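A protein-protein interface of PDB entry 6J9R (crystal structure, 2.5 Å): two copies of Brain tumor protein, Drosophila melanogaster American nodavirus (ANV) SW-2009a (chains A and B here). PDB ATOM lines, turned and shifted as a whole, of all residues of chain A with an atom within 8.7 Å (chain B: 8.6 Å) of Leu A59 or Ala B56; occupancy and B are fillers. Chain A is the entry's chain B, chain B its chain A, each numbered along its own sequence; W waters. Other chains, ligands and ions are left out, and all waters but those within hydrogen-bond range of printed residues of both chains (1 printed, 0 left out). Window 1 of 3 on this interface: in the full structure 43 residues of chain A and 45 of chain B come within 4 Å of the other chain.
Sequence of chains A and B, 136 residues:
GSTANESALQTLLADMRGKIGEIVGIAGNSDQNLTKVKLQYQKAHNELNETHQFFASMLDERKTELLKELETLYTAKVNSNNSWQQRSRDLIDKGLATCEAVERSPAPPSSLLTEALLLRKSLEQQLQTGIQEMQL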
ATOM      1  N   HIS A  52      -5.001  21.790 -10.785  1.00  0.00           N
ATOM      2  CA  HIS A  52      -4.824  21.746  -9.347  1.00  0.00           C
ATOM      3  C   HIS A  52      -3.482  22.319  -8.944  1.00  0.00           C
ATOM      4  O   HIS A  52      -3.384  23.041  -7.973  1.00  0.00           O
ATOM      5  CB  HIS A  52      -4.919  20.322  -8.816  1.00  0.00           C
ATOM      6  CG  HIS A  52      -4.494  20.213  -7.389  1.00  0.00           C
ATOM      7  ND1 HIS A  52      -3.228  19.813  -7.025  1.00  0.00           N
ATOM      8  CD2 HIS A  52      -5.148  20.507  -6.242  1.00  0.00           C
ATOM      9  CE1 HIS A  52      -3.124  19.846  -5.703  1.00  0.00           C
ATOM     10  NE2 HIS A  52      -4.273  20.259  -5.207  1.00  0.00           N
ATOM     11  N   GLN A  53      -2.447  21.957  -9.693  1.00  0.00           N
ATOM     12  CA  GLN A  53      -1.109  22.412  -9.405  1.00  0.00           C
ATOM     13  C   GLN A  53      -0.970  23.900  -9.654  1.00  0.00           C
ATOM     14  O   GLN A  53      -0.318  24.622  -8.887  1.00  0.00           O
ATOM     15  CB  GLN A  53      -0.115  21.640 -10.254  1.00  0.00           C
ATOM     16  CG  GLN A  53       1.300  21.922  -9.919  1.00  0.00           C
ATOM     17  CD  GLN A  53       2.206  21.096 -10.764  1.00  0.00           C
ATOM     18  OE1 GLN A  53       2.635  20.021 -10.359  1.00  0.00           O
ATOM     19  NE2 GLN A  53       2.482  21.570 -11.965  1.00  0.00           N
ATOM     20  N   PHE A  54      -1.636  24.366 -10.697  1.00  0.00           N
ATOM     21  CA  PHE A  54      -1.646  25.784 -10.971  1.00  0.00           C
ATOM     22  C   PHE A  54      -2.309  26.568  -9.820  1.00  0.00           C
ATOM     23  O   PHE A  54      -1.714  27.545  -9.322  1.00  0.00           O
ATOM     24  CB  PHE A  54      -2.353  26.074 -12.285  1.00  0.00           C
ATOM     25  CG  PHE A  54      -2.742  27.502 -12.433  1.00  0.00           C
ATOM     26  CD1 PHE A  54      -1.789  28.462 -12.737  1.00  0.00           C
ATOM     27  CD2 PHE A  54      -4.053  27.896 -12.213  1.00  0.00           C
ATOM     28  CE1 PHE A  54      -2.120  29.780 -12.841  1.00  0.00           C
ATOM     29  CE2 PHE A  54      -4.402  29.221 -12.318  1.00  0.00           C
ATOM     30  CZ  PHE A  54      -3.426  30.175 -12.639  1.00  0.00           C
ATOM     31  N   PHE A  55      -3.482  26.130  -9.346  1.00  0.00           N
ATOM     32  CA  PHE A  55      -4.133  26.870  -8.268  1.00  0.00           C
ATOM     33  C   PHE A  55      -3.410  26.740  -6.943  1.00  0.00           C
ATOM     34  O   PHE A  55      -3.453  27.642  -6.129  1.00  0.00           O
ATOM     35  CB  PHE A  55      -5.582  26.440  -8.080  1.00  0.00           C
ATOM     36  CG  PHE A  55      -6.489  27.038  -9.078  1.00  0.00           C
ATOM     37  CD1 PHE A  55      -6.702  28.413  -9.084  1.00  0.00           C
ATOM     38  CD2 PHE A  55      -7.085  26.249 -10.064  1.00  0.00           C
ATOM     39  CE1 PHE A  55      -7.528  28.981 -10.057  1.00  0.00           C
ATOM     40  CE2 PHE A  55      -7.897  26.803 -11.025  1.00  0.00           C
ATOM     41  CZ  PHE A  55      -8.127  28.163 -11.028  1.00  0.00           C
ATOM     42  N   ALA A  56      -2.714  25.639  -6.740  1.00  0.00           N
ATOM     43  CA  ALA A  56      -1.989  25.462  -5.502  1.00  0.00           C
ATOM     44  C   ALA A  56      -0.861  26.481  -5.482  1.00  0.00           C
ATOM     45  O   ALA A  56      -0.629  27.103  -4.458  1.00  0.00           O
ATOM     46  CB  ALA A  56      -1.461  24.033  -5.362  1.00  0.00           C
ATOM     47  N   SER A  57      -0.211  26.704  -6.623  1.00  0.00           N
ATOM     48  CA  SER A  57       0.855  27.687  -6.639  1.00  0.00           C
ATOM     49  C   SER A  57       0.288  29.099  -6.470  1.00  0.00           C
ATOM     50  O   SER A  57       0.902  29.927  -5.781  1.00  0.00           O
ATOM     51  CB  SER A  57       1.718  27.561  -7.898  1.00  0.00           C
ATOM     52  OG  SER A  57       1.056  27.976  -9.068  1.00  0.00           O
ATOM     53  N   MET A  58      -0.885  29.354  -7.052  1.00  0.00           N
ATOM     54  CA  MET A  58      -1.581  30.625  -6.867  1.00  0.00           C
ATOM     55  C   MET A  58      -1.926  30.843  -5.404  1.00  0.00           C
ATOM     56  O   MET A  58      -1.863  31.949  -4.898  1.00  0.00           O
ATOM     57  CB  MET A  58      -2.868  30.680  -7.693  1.00  0.00           C
ATOM     58  CG  MET A  58      -2.662  30.777  -9.190  1.00  0.00           C
ATOM     59  SD  MET A  58      -1.536  32.269  -9.786  1.00  0.00           S
ATOM     60  CE  MET A  58      -0.008  31.208 -10.351  1.00  0.00           C
ATOM     61  N   LEU A  59      -2.312  29.771  -4.739  1.00  0.00           N
ATOM     62  CA  LEU A  59      -2.648  29.833  -3.344  1.00  0.00           C
ATOM     63  C   LEU A  59      -1.405  30.133  -2.491  1.00  0.00           C
ATOM     64  O   LEU A  59      -1.481  30.880  -1.502  1.00  0.00           O
ATOM     65  CB  LEU A  59      -3.287  28.518  -2.930  1.00  0.00           C
ATOM     66  CG  LEU A  59      -3.919  28.421  -1.556  1.00  0.00           C
ATOM     67  CD1 LEU A  59      -5.097  29.388  -1.469  1.00  0.00           C
ATOM     68  CD2 LEU A  59      -4.342  26.979  -1.314  1.00  0.00           C
ATOM     69  N   ASP A  60      -0.260  29.560  -2.863  1.00  0.00           N
ATOM     70  CA  ASP A  60       0.964  29.862  -2.130  1.00  0.00           C
ATOM     71  C   ASP A  60       1.305  31.320  -2.334  1.00  0.00           C
ATOM     72  O   ASP A  60       1.616  31.995  -1.373  1.00  0.00           O
ATOM     73  CB  ASP A  60       2.146  28.980  -2.526  1.00  0.00           C
ATOM     74  CG  ASP A  60       1.973  27.538  -2.091  1.00  0.00           C
ATOM     75  OD1 ASP A  60       1.081  27.258  -1.241  1.00  0.00           O
ATOM     76  OD2 ASP A  60       2.757  26.687  -2.577  1.00  0.00           O
ATOM     77  N   GLU A  61       1.213  31.812  -3.570  1.00  0.00           N
ATOM     78  CA  GLU A  61       1.547  33.212  -3.829  1.00  0.00           C
ATOM     79  C   GLU A  61       0.668  34.166  -2.990  1.00  0.00           C
ATOM     80  O   GLU A  61       1.148  35.142  -2.402  1.00  0.00           O
ATOM     81  CB  GLU A  61       1.398  33.542  -5.322  1.00  0.00           C
ATOM     82  CG  GLU A  61       1.504  35.044  -5.642  1.00  0.00           C
ATOM     83  CD  GLU A  61       2.795  35.687  -5.123  1.00  0.00           C
ATOM     84  OE1 GLU A  61       3.800  34.980  -4.952  1.00  0.00           O
ATOM     85  OE2 GLU A  61       2.811  36.909  -4.869  1.00  0.00           O
ATOM     86  N   ARG A  62      -0.602  33.838  -2.880  1.00  0.00           N
ATOM     87  CA  ARG A  62      -1.475  34.641  -2.079  1.00  0.00           C
ATOM     88  C   ARG A  62      -1.062  34.613  -0.626  1.00  0.00           C
ATOM     89  O   ARG A  62      -1.106  35.632   0.062  1.00  0.00           O
ATOM     90  CB  ARG A  62      -2.923  34.171  -2.208  1.00  0.00           C
ATOM     91  CG  ARG A  62      -3.885  35.178  -1.606  1.00  0.00           C
ATOM     92  CD  ARG A  62      -3.747  36.564  -2.255  1.00  0.00           C
ATOM     93  NE  ARG A  62      -4.630  37.545  -1.615  1.00  0.00           N
ATOM     94  CZ  ARG A  62      -4.301  38.816  -1.384  1.00  0.00           C
ATOM     95  NH1 ARG A  62      -3.117  39.282  -1.759  1.00  0.00           N
ATOM     96  NH2 ARG A  62      -5.160  39.628  -0.780  1.00  0.00           N
ATOM     97  N   LYS A  63      -0.645  33.451  -0.155  1.00  0.00           N
ATOM     98  CA  LYS A  63      -0.261  33.353   1.232  1.00  0.00           C
ATOM     99  C   LYS A  63       0.961  34.209   1.477  1.00  0.00           C
ATOM    100  O   LYS A  63       1.006  34.936   2.463  1.00  0.00           O
ATOM    101  CB  LYS A  63      -0.009  31.918   1.658  1.00  0.00           C
ATOM    102  CG  LYS A  63       0.454  31.821   3.098  1.00  0.00           C
ATOM    103  CD  LYS A  63       1.071  30.506   3.369  1.00  0.00           C
ATOM    104  CE  LYS A  63       1.703  30.491   4.743  1.00  0.00           C
ATOM    105  NZ  LYS A  63       1.997  29.089   5.139  1.00  0.00           N
ATOM    106  N   THR A  64       1.931  34.169   0.569  1.00  0.00           N
ATOM    107  CA  THR A  64       3.120  34.932   0.843  1.00  0.00           C
ATOM    108  C   THR A  64       2.833  36.452   0.746  1.00  0.00           C
ATOM    109  O   THR A  64       3.431  37.197   1.482  1.00  0.00           O
ATOM    110  CB  THR A  64       4.338  34.494  -0.070  1.00  0.00           C
ATOM    111  OG1 THR A  64       4.451  35.293  -1.246  1.00  0.00           O
ATOM    112  CG2 THR A  64       4.250  33.036  -0.414  1.00  0.00           C
ATOM    113  N   GLU A  65       1.896  36.902  -0.096  1.00  0.00           N
ATOM    114  CA  GLU A  65       1.499  38.326  -0.098  1.00  0.00           C
ATOM    115  C   GLU A  65       0.844  38.756   1.218  1.00  0.00           C
ATOM    116  O   GLU A  65       1.189  39.793   1.787  1.00  0.00           O
ATOM    117  CB  GLU A  65       0.510  38.631  -1.237  1.00  0.00           C
ATOM    118  CG  GLU A  65       1.107  38.552  -2.640  1.00  0.00           C
ATOM    119  CD  GLU A  65       0.067  38.336  -3.739  1.00  0.00           C
ATOM    120  OE1 GLU A  65       0.466  38.097  -4.899  1.00  0.00           O
ATOM    121  OE2 GLU A  65      -1.146  38.400  -3.452  1.00  0.00           O
ATOM    122  N   LEU A  66      -0.072  37.933   1.713  1.00  0.00           N
ATOM    123  CA  LEU A  66      -0.773  38.227   2.953  1.00  0.00           C
ATOM    124  C   LEU A  66       0.215  38.233   4.106  1.00  0.00           C
ATOM    125  O   LEU A  66       0.151  39.099   4.982  1.00  0.00           O
ATOM    126  CB  LEU A  66      -1.877  37.192   3.202  1.00  0.00           C
ATOM    127  CG  LEU A  66      -3.128  37.276   2.320  1.00  0.00           C
ATOM    128  CD1 LEU A  66      -4.115  36.135   2.632  1.00  0.00           C
ATOM    129  CD2 LEU A  66      -3.816  38.621   2.492  1.00  0.00           C
ATOM    130  N   LEU B  48      -3.546  32.893   9.588  1.00  0.00           N
ATOM    131  CA  LEU B  48      -3.226  32.908   8.191  1.00  0.00           C
ATOM    132  C   LEU B  48      -2.788  31.499   7.747  1.00  0.00           C
ATOM    133  O   LEU B  48      -3.177  31.048   6.673  1.00  0.00           O
ATOM    134  CB  LEU B  48      -2.144  33.962   7.908  1.00  0.00           C
ATOM    135  CG  LEU B  48      -1.601  33.913   6.474  1.00  0.00           C
ATOM    136  CD1 LEU B  48      -2.757  33.979   5.436  1.00  0.00           C
ATOM    137  CD2 LEU B  48      -0.575  35.011   6.245  1.00  0.00           C
ATOM    138  N   ASN B  49      -2.041  30.789   8.593  1.00  0.00           N
ATOM    139  CA  ASN B  49      -1.503  29.475   8.219  1.00  0.00           C
ATOM    140  C   ASN B  49      -2.590  28.421   8.221  1.00  0.00           C
ATOM    141  O   ASN B  49      -2.636  27.548   7.354  1.00  0.00           O
ATOM    142  CB  ASN B  49      -0.366  29.059   9.168  1.00  0.00           C
ATOM    143  CG  ASN B  49       0.952  29.762   8.849  1.00  0.00           C
ATOM    144  OD1 ASN B  49       1.091  30.400   7.814  1.00  0.00           O
ATOM    145  ND2 ASN B  49       1.900  29.694   9.768  1.00  0.00           N
ATOM    146  N   GLU B  50      -3.485  28.527   9.191  1.00  0.00           N
ATOM    147  CA  GLU B  50      -4.601  27.598   9.304  1.00  0.00           C
ATOM    148  C   GLU B  50      -5.491  27.732   8.103  1.00  0.00           C
ATOM    149  O   GLU B  50      -5.926  26.732   7.516  1.00  0.00           O
ATOM    150  CB  GLU B  50      -5.407  27.877  10.561  1.00  0.00           C
ATOM    151  CG  GLU B  50      -4.722  27.519  11.850  1.00  0.00           C
ATOM    152  CD  GLU B  50      -5.586  27.863  13.044  1.00  0.00           C
ATOM    153  OE1 GLU B  50      -6.797  28.148  12.839  1.00  0.00           O
ATOM    154  OE2 GLU B  50      -5.053  27.846  14.178  1.00  0.00           O
ATOM    155  N   THR B  51      -5.768  28.987   7.753  1.00  0.00           N
ATOM    156  CA  THR B  51      -6.632  29.295   6.627  1.00  0.00           C
ATOM    157  C   THR B  51      -6.045  28.808   5.321  1.00  0.00           C
ATOM    158  O   THR B  51      -6.753  28.201   4.507  1.00  0.00           O
ATOM    159  CB  THR B  51      -6.890  30.800   6.529  1.00  0.00           C
ATOM    160  OG1 THR B  51      -7.735  31.170   7.615  1.00  0.00           O
ATOM    161  CG2 THR B  51      -7.617  31.155   5.228  1.00  0.00           C
ATOM    162  N   HIS B  52      -4.751  29.044   5.139  1.00  0.00           N
ATOM    163  CA  HIS B  52      -4.114  28.584   3.934  1.00  0.00           C
ATOM    164  C   HIS B  52      -4.155  27.071   3.893  1.00  0.00           C
ATOM    165  O   HIS B  52      -4.491  26.479   2.872  1.00  0.00           O
ATOM    166  CB  HIS B  52      -2.673  29.061   3.839  1.00  0.00           C
ATOM    167  CG  HIS B  52      -1.937  28.449   2.695  1.00  0.00           C
ATOM    168  ND1 HIS B  52      -1.098  27.366   2.838  1.00  0.00           N
ATOM    169  CD2 HIS B  52      -1.950  28.740   1.371  1.00  0.00           C
ATOM    170  CE1 HIS B  52      -0.599  27.035   1.661  1.00  0.00           C
ATOM    171  NE2 HIS B  52      -1.101  27.855   0.753  1.00  0.00           N
ATOM    172  N   GLN B  53      -3.854  26.457   5.034  1.00  0.00           N
ATOM    173  CA  GLN B  53      -3.840  25.016   5.115  1.00  0.00           C
ATOM    174  C   GLN B  53      -5.242  24.470   4.905  1.00  0.00           C
ATOM    175  O   GLN B  53      -5.414  23.415   4.302  1.00  0.00           O
ATOM    176  CB  GLN B  53      -3.279  24.539   6.450  1.00  0.00           C
ATOM    177  CG  GLN B  53      -3.104  23.039   6.510  1.00  0.00           C
ATOM    178  CD  GLN B  53      -2.333  22.514   5.315  1.00  0.00           C
ATOM    179  OE1 GLN B  53      -1.376  23.144   4.855  1.00  0.00           O
ATOM    180  NE2 GLN B  53      -2.760  21.370   4.786  1.00  0.00           N
ATOM    181  N   PHE B  54      -6.249  25.202   5.367  1.00  0.00           N
ATOM    182  CA  PHE B  54      -7.623  24.760   5.135  1.00  0.00           C
ATOM    183  C   PHE B  54      -7.981  24.736   3.619  1.00  0.00           C
ATOM    184  O   PHE B  54      -8.581  23.771   3.116  1.00  0.00           O
ATOM    185  CB  PHE B  54      -8.625  25.628   5.917  1.00  0.00           C
ATOM    186  CG  PHE B  54     -10.044  25.393   5.507  1.00  0.00           C
ATOM    187  CD1 PHE B  54     -10.724  24.249   5.938  1.00  0.00           C
ATOM    188  CD2 PHE B  54     -10.684  26.260   4.637  1.00  0.00           C
ATOM    189  CE1 PHE B  54     -12.007  23.989   5.530  1.00  0.00           C
ATOM    190  CE2 PHE B  54     -11.978  26.016   4.230  1.00  0.00           C
ATOM    191  CZ  PHE B  54     -12.642  24.877   4.673  1.00  0.00           C
ATOM    192  N   PHE B  55      -7.630  25.788   2.884  1.00  0.00           N
ATOM    193  CA  PHE B  55      -7.988  25.813   1.467  1.00  0.00           C
ATOM    194  C   PHE B  55      -7.129  24.864   0.658  1.00  0.00           C
ATOM    195  O   PHE B  55      -7.587  24.328  -0.350  1.00  0.00           O
ATOM    196  CB  PHE B  55      -7.876  27.224   0.914  1.00  0.00           C
ATOM    197  CG  PHE B  55      -9.013  28.109   1.325  1.00  0.00           C
ATOM    198  CD1 PHE B  55     -10.298  27.891   0.839  1.00  0.00           C
ATOM    199  CD2 PHE B  55      -8.811  29.113   2.244  1.00  0.00           C
ATOM    200  CE1 PHE B  55     -11.359  28.702   1.236  1.00  0.00           C
ATOM    201  CE2 PHE B  55      -9.867  29.929   2.654  1.00  0.00           C
ATOM    202  CZ  PHE B  55     -11.136  29.726   2.149  1.00  0.00           C
ATOM    203  N   ALA B  56      -5.896  24.625   1.104  1.00  0.00           N
ATOM    204  CA  ALA B  56      -5.032  23.708   0.378  1.00  0.00           C
ATOM    205  C   ALA B  56      -5.562  22.292   0.537  1.00  0.00           C
ATOM    206  O   ALA B  56      -5.592  21.532  -0.427  1.00  0.00           O
ATOM    207  CB  ALA B  56      -3.593  23.815   0.853  1.00  0.00           C
ATOM    208  N   SER B  57      -6.036  21.943   1.729  1.00  0.00           N
ATOM    209  CA  SER B  57      -6.582  20.603   1.928  1.00  0.00           C
ATOM    210  C   SER B  57      -7.854  20.429   1.113  1.00  0.00           C
ATOM    211  O   SER B  57      -8.072  19.380   0.505  1.00  0.00           O
ATOM    212  CB  SER B  57      -6.855  20.334   3.405  1.00  0.00           C
ATOM    213  OG  SER B  57      -5.625  20.276   4.117  1.00  0.00           O
ATOM    214  N   MET B  58      -8.661  21.486   1.093  1.00  0.00           N
ATOM    215  CA  MET B  58      -9.852  21.602   0.259  1.00  0.00           C
ATOM    216  C   MET B  58      -9.545  21.329  -1.220  1.00  0.00           C
ATOM    217  O   MET B  58     -10.147  20.467  -1.847  1.00  0.00           O
ATOM    218  CB  MET B  58     -10.435  22.995   0.427  1.00  0.00           C
ATOM    219  CG  MET B  58     -11.781  23.236  -0.186  1.00  0.00           C
ATOM    220  SD  MET B  58     -12.971  23.742   1.265  1.00  0.00           S
ATOM    221  CE  MET B  58     -13.031  21.987   2.073  1.00  0.00           C
ATOM    222  N   LEU B  59      -8.588  22.053  -1.774  1.00  0.00           N
ATOM    223  CA  LEU B  59      -8.228  21.841  -3.157  1.00  0.00           C
ATOM    224  C   LEU B  59      -7.687  20.423  -3.402  1.00  0.00           C
ATOM    225  O   LEU B  59      -8.023  19.818  -4.412  1.00  0.00           O
ATOM    226  CB  LEU B  59      -7.213  22.886  -3.613  1.00  0.00           C
ATOM    227  CG  LEU B  59      -7.780  24.304  -3.745  1.00  0.00           C
ATOM    228  N   ASP B  60      -6.930  19.867  -2.462  1.00  0.00           N
ATOM    229  CA  ASP B  60      -6.392  18.527  -2.659  1.00  0.00           C
ATOM    230  C   ASP B  60      -7.514  17.501  -2.712  1.00  0.00           C
ATOM    231  O   ASP B  60      -7.625  16.704  -3.637  1.00  0.00           O
ATOM    232  CB  ASP B  60      -5.439  18.151  -1.519  1.00  0.00           C
ATOM    233  CG  ASP B  60      -4.196  19.033  -1.464  1.00  0.00           C
ATOM    234  OD1 ASP B  60      -3.880  19.709  -2.475  1.00  0.00           O
ATOM    235  OD2 ASP B  60      -3.553  19.089  -0.379  1.00  0.00           O
ATOM    236  N   GLU B  61      -8.369  17.568  -1.699  1.00  0.00           N
ATOM    237  CA  GLU B  61      -9.450  16.631  -1.532  1.00  0.00           C
ATOM    238  C   GLU B  61     -10.412  16.692  -2.695  1.00  0.00           C
ATOM    239  O   GLU B  61     -10.868  15.664  -3.173  1.00  0.00           O
ATOM    240  CB  GLU B  61     -10.149  16.895  -0.203  1.00  0.00           C
ATOM    241  CG  GLU B  61      -9.335  16.385   0.964  1.00  0.00           C
ATOM    242  CD  GLU B  61      -9.643  17.094   2.263  1.00  0.00           C
ATOM    243  OE1 GLU B  61     -10.688  17.778   2.337  1.00  0.00           O
ATOM    244  OE2 GLU B  61      -8.832  16.972   3.211  1.00  0.00           O
ATOM    245  N   ARG B  62     -10.692  17.893  -3.173  1.00  0.00           N
ATOM    246  CA  ARG B  62     -11.585  18.056  -4.299  1.00  0.00           C
ATOM    247  C   ARG B  62     -10.967  17.403  -5.546  1.00  0.00           C
ATOM    248  O   ARG B  62     -11.654  16.691  -6.302  1.00  0.00           O
ATOM    249  CB  ARG B  62     -11.869  19.544  -4.520  1.00  0.00           C
ATOM    250  CG  ARG B  62     -13.074  19.836  -5.399  1.00  0.00           C
ATOM    251  CD  ARG B  62     -12.672  20.041  -6.847  1.00  0.00           C
ATOM    252  N   LYS B  63      -9.656  17.588  -5.710  1.00  0.00           N
ATOM    253  CA  LYS B  63      -8.950  17.000  -6.825  1.00  0.00           C
ATOM    254  C   LYS B  63      -9.000  15.489  -6.829  1.00  0.00           C
ATOM    255  O   LYS B  63      -9.263  14.887  -7.875  1.00  0.00           O
ATOM    256  CB  LYS B  63      -7.492  17.416  -6.811  1.00  0.00           C
ATOM    257  CG  LYS B  63      -6.621  16.615  -7.796  1.00  0.00           C
ATOM    258  CD  LYS B  63      -5.183  16.619  -7.262  1.00  0.00           C
ATOM    259  CE  LYS B  63      -4.329  15.631  -7.971  1.00  0.00           C
ATOM    260  NZ  LYS B  63      -2.882  15.841  -7.709  1.00  0.00           N
HETATM  261  O   HOH W   1      -0.975  25.802  -1.748  1.00  0.00           O
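Among the printed residues, merely in contact across the chains: His A52 with Leu B59 (3.5 Å), His A52 with Lys B63 (3.7 Å), Leu A59 with His B52 (3.5 Å), Leu A59 with Ala B56 (3.7 Å), Lys A63 with His B52 (3.7 Å) and Leu A66 with Leu B48 (3.8 Å).
Water W1 lies within hydrogen-bond range of OD1 of Asp A60 (2.6 Å), O of Ala A56 (3.0 Å) and NE2 of His B52 (3.2 Å).
Of the 15 printed residues of chain A, 5 touch a printed residue of chain B.
Hydrophobic or aromatic side chains of chain A within 4 Å of the printed part of chain B: His A52, Leu A59 and Leu A66.
Along chain A the printed residues that touch a printed residue of chain B span positions 52 to 66.
Of the 16 printed residues of chain B, 7 touch a printed residue of chain A.
OD1 of Asp B60 sits at hydrogen-bond distance from NE2 of His A52, 2.8 Å away.
NE2 of His B52 lies within hydrogen-bond range of OD1 of Asp A60, 3.0 Å away.
The side-chain amide oxygen of Asn B49 lies within hydrogen-bond range of the side-chain amino group of Lys A63 (3.1 Å).
Of the printed residues of chain B, His A52 touches Leu B59, Asp B60 and Lys B63.
Of the printed residues of chain B, Leu A59 touches His B52 (3.5 Å) and Ala B56 (3.7 Å).
Of the printed residues of chain B, Asp A60 touches His B52 (3.0 Å).
Glu A65 touches none of the printed residues of chain B.
No residue of chain A comes within 4 Å of Ser B57.
The nearest residue of chain A that does not touch Ala B56 is His A52 (5.1 Å).
The nearest printed residue of chain A that does not touch His B52 is Ala A56 (5.3 Å).
His A52 touches Leu B59, and with the chains exchanged Leu A59 touches His B52.
His A52 touches Asp B60, and with the chains exchanged Asp A60 touches His B52.
His A52 touches Lys B63, and with the chains exchanged Lys A63 touches His B52.
Leu A59 touches Ala B56, but with the chains exchanged Ala A56 does not touch Leu B59 (6.0 Å).
Positions printed for both chains: 52, 53, 54, 55, 56, 57, 58, 59, 60, 61, 62 and 63.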
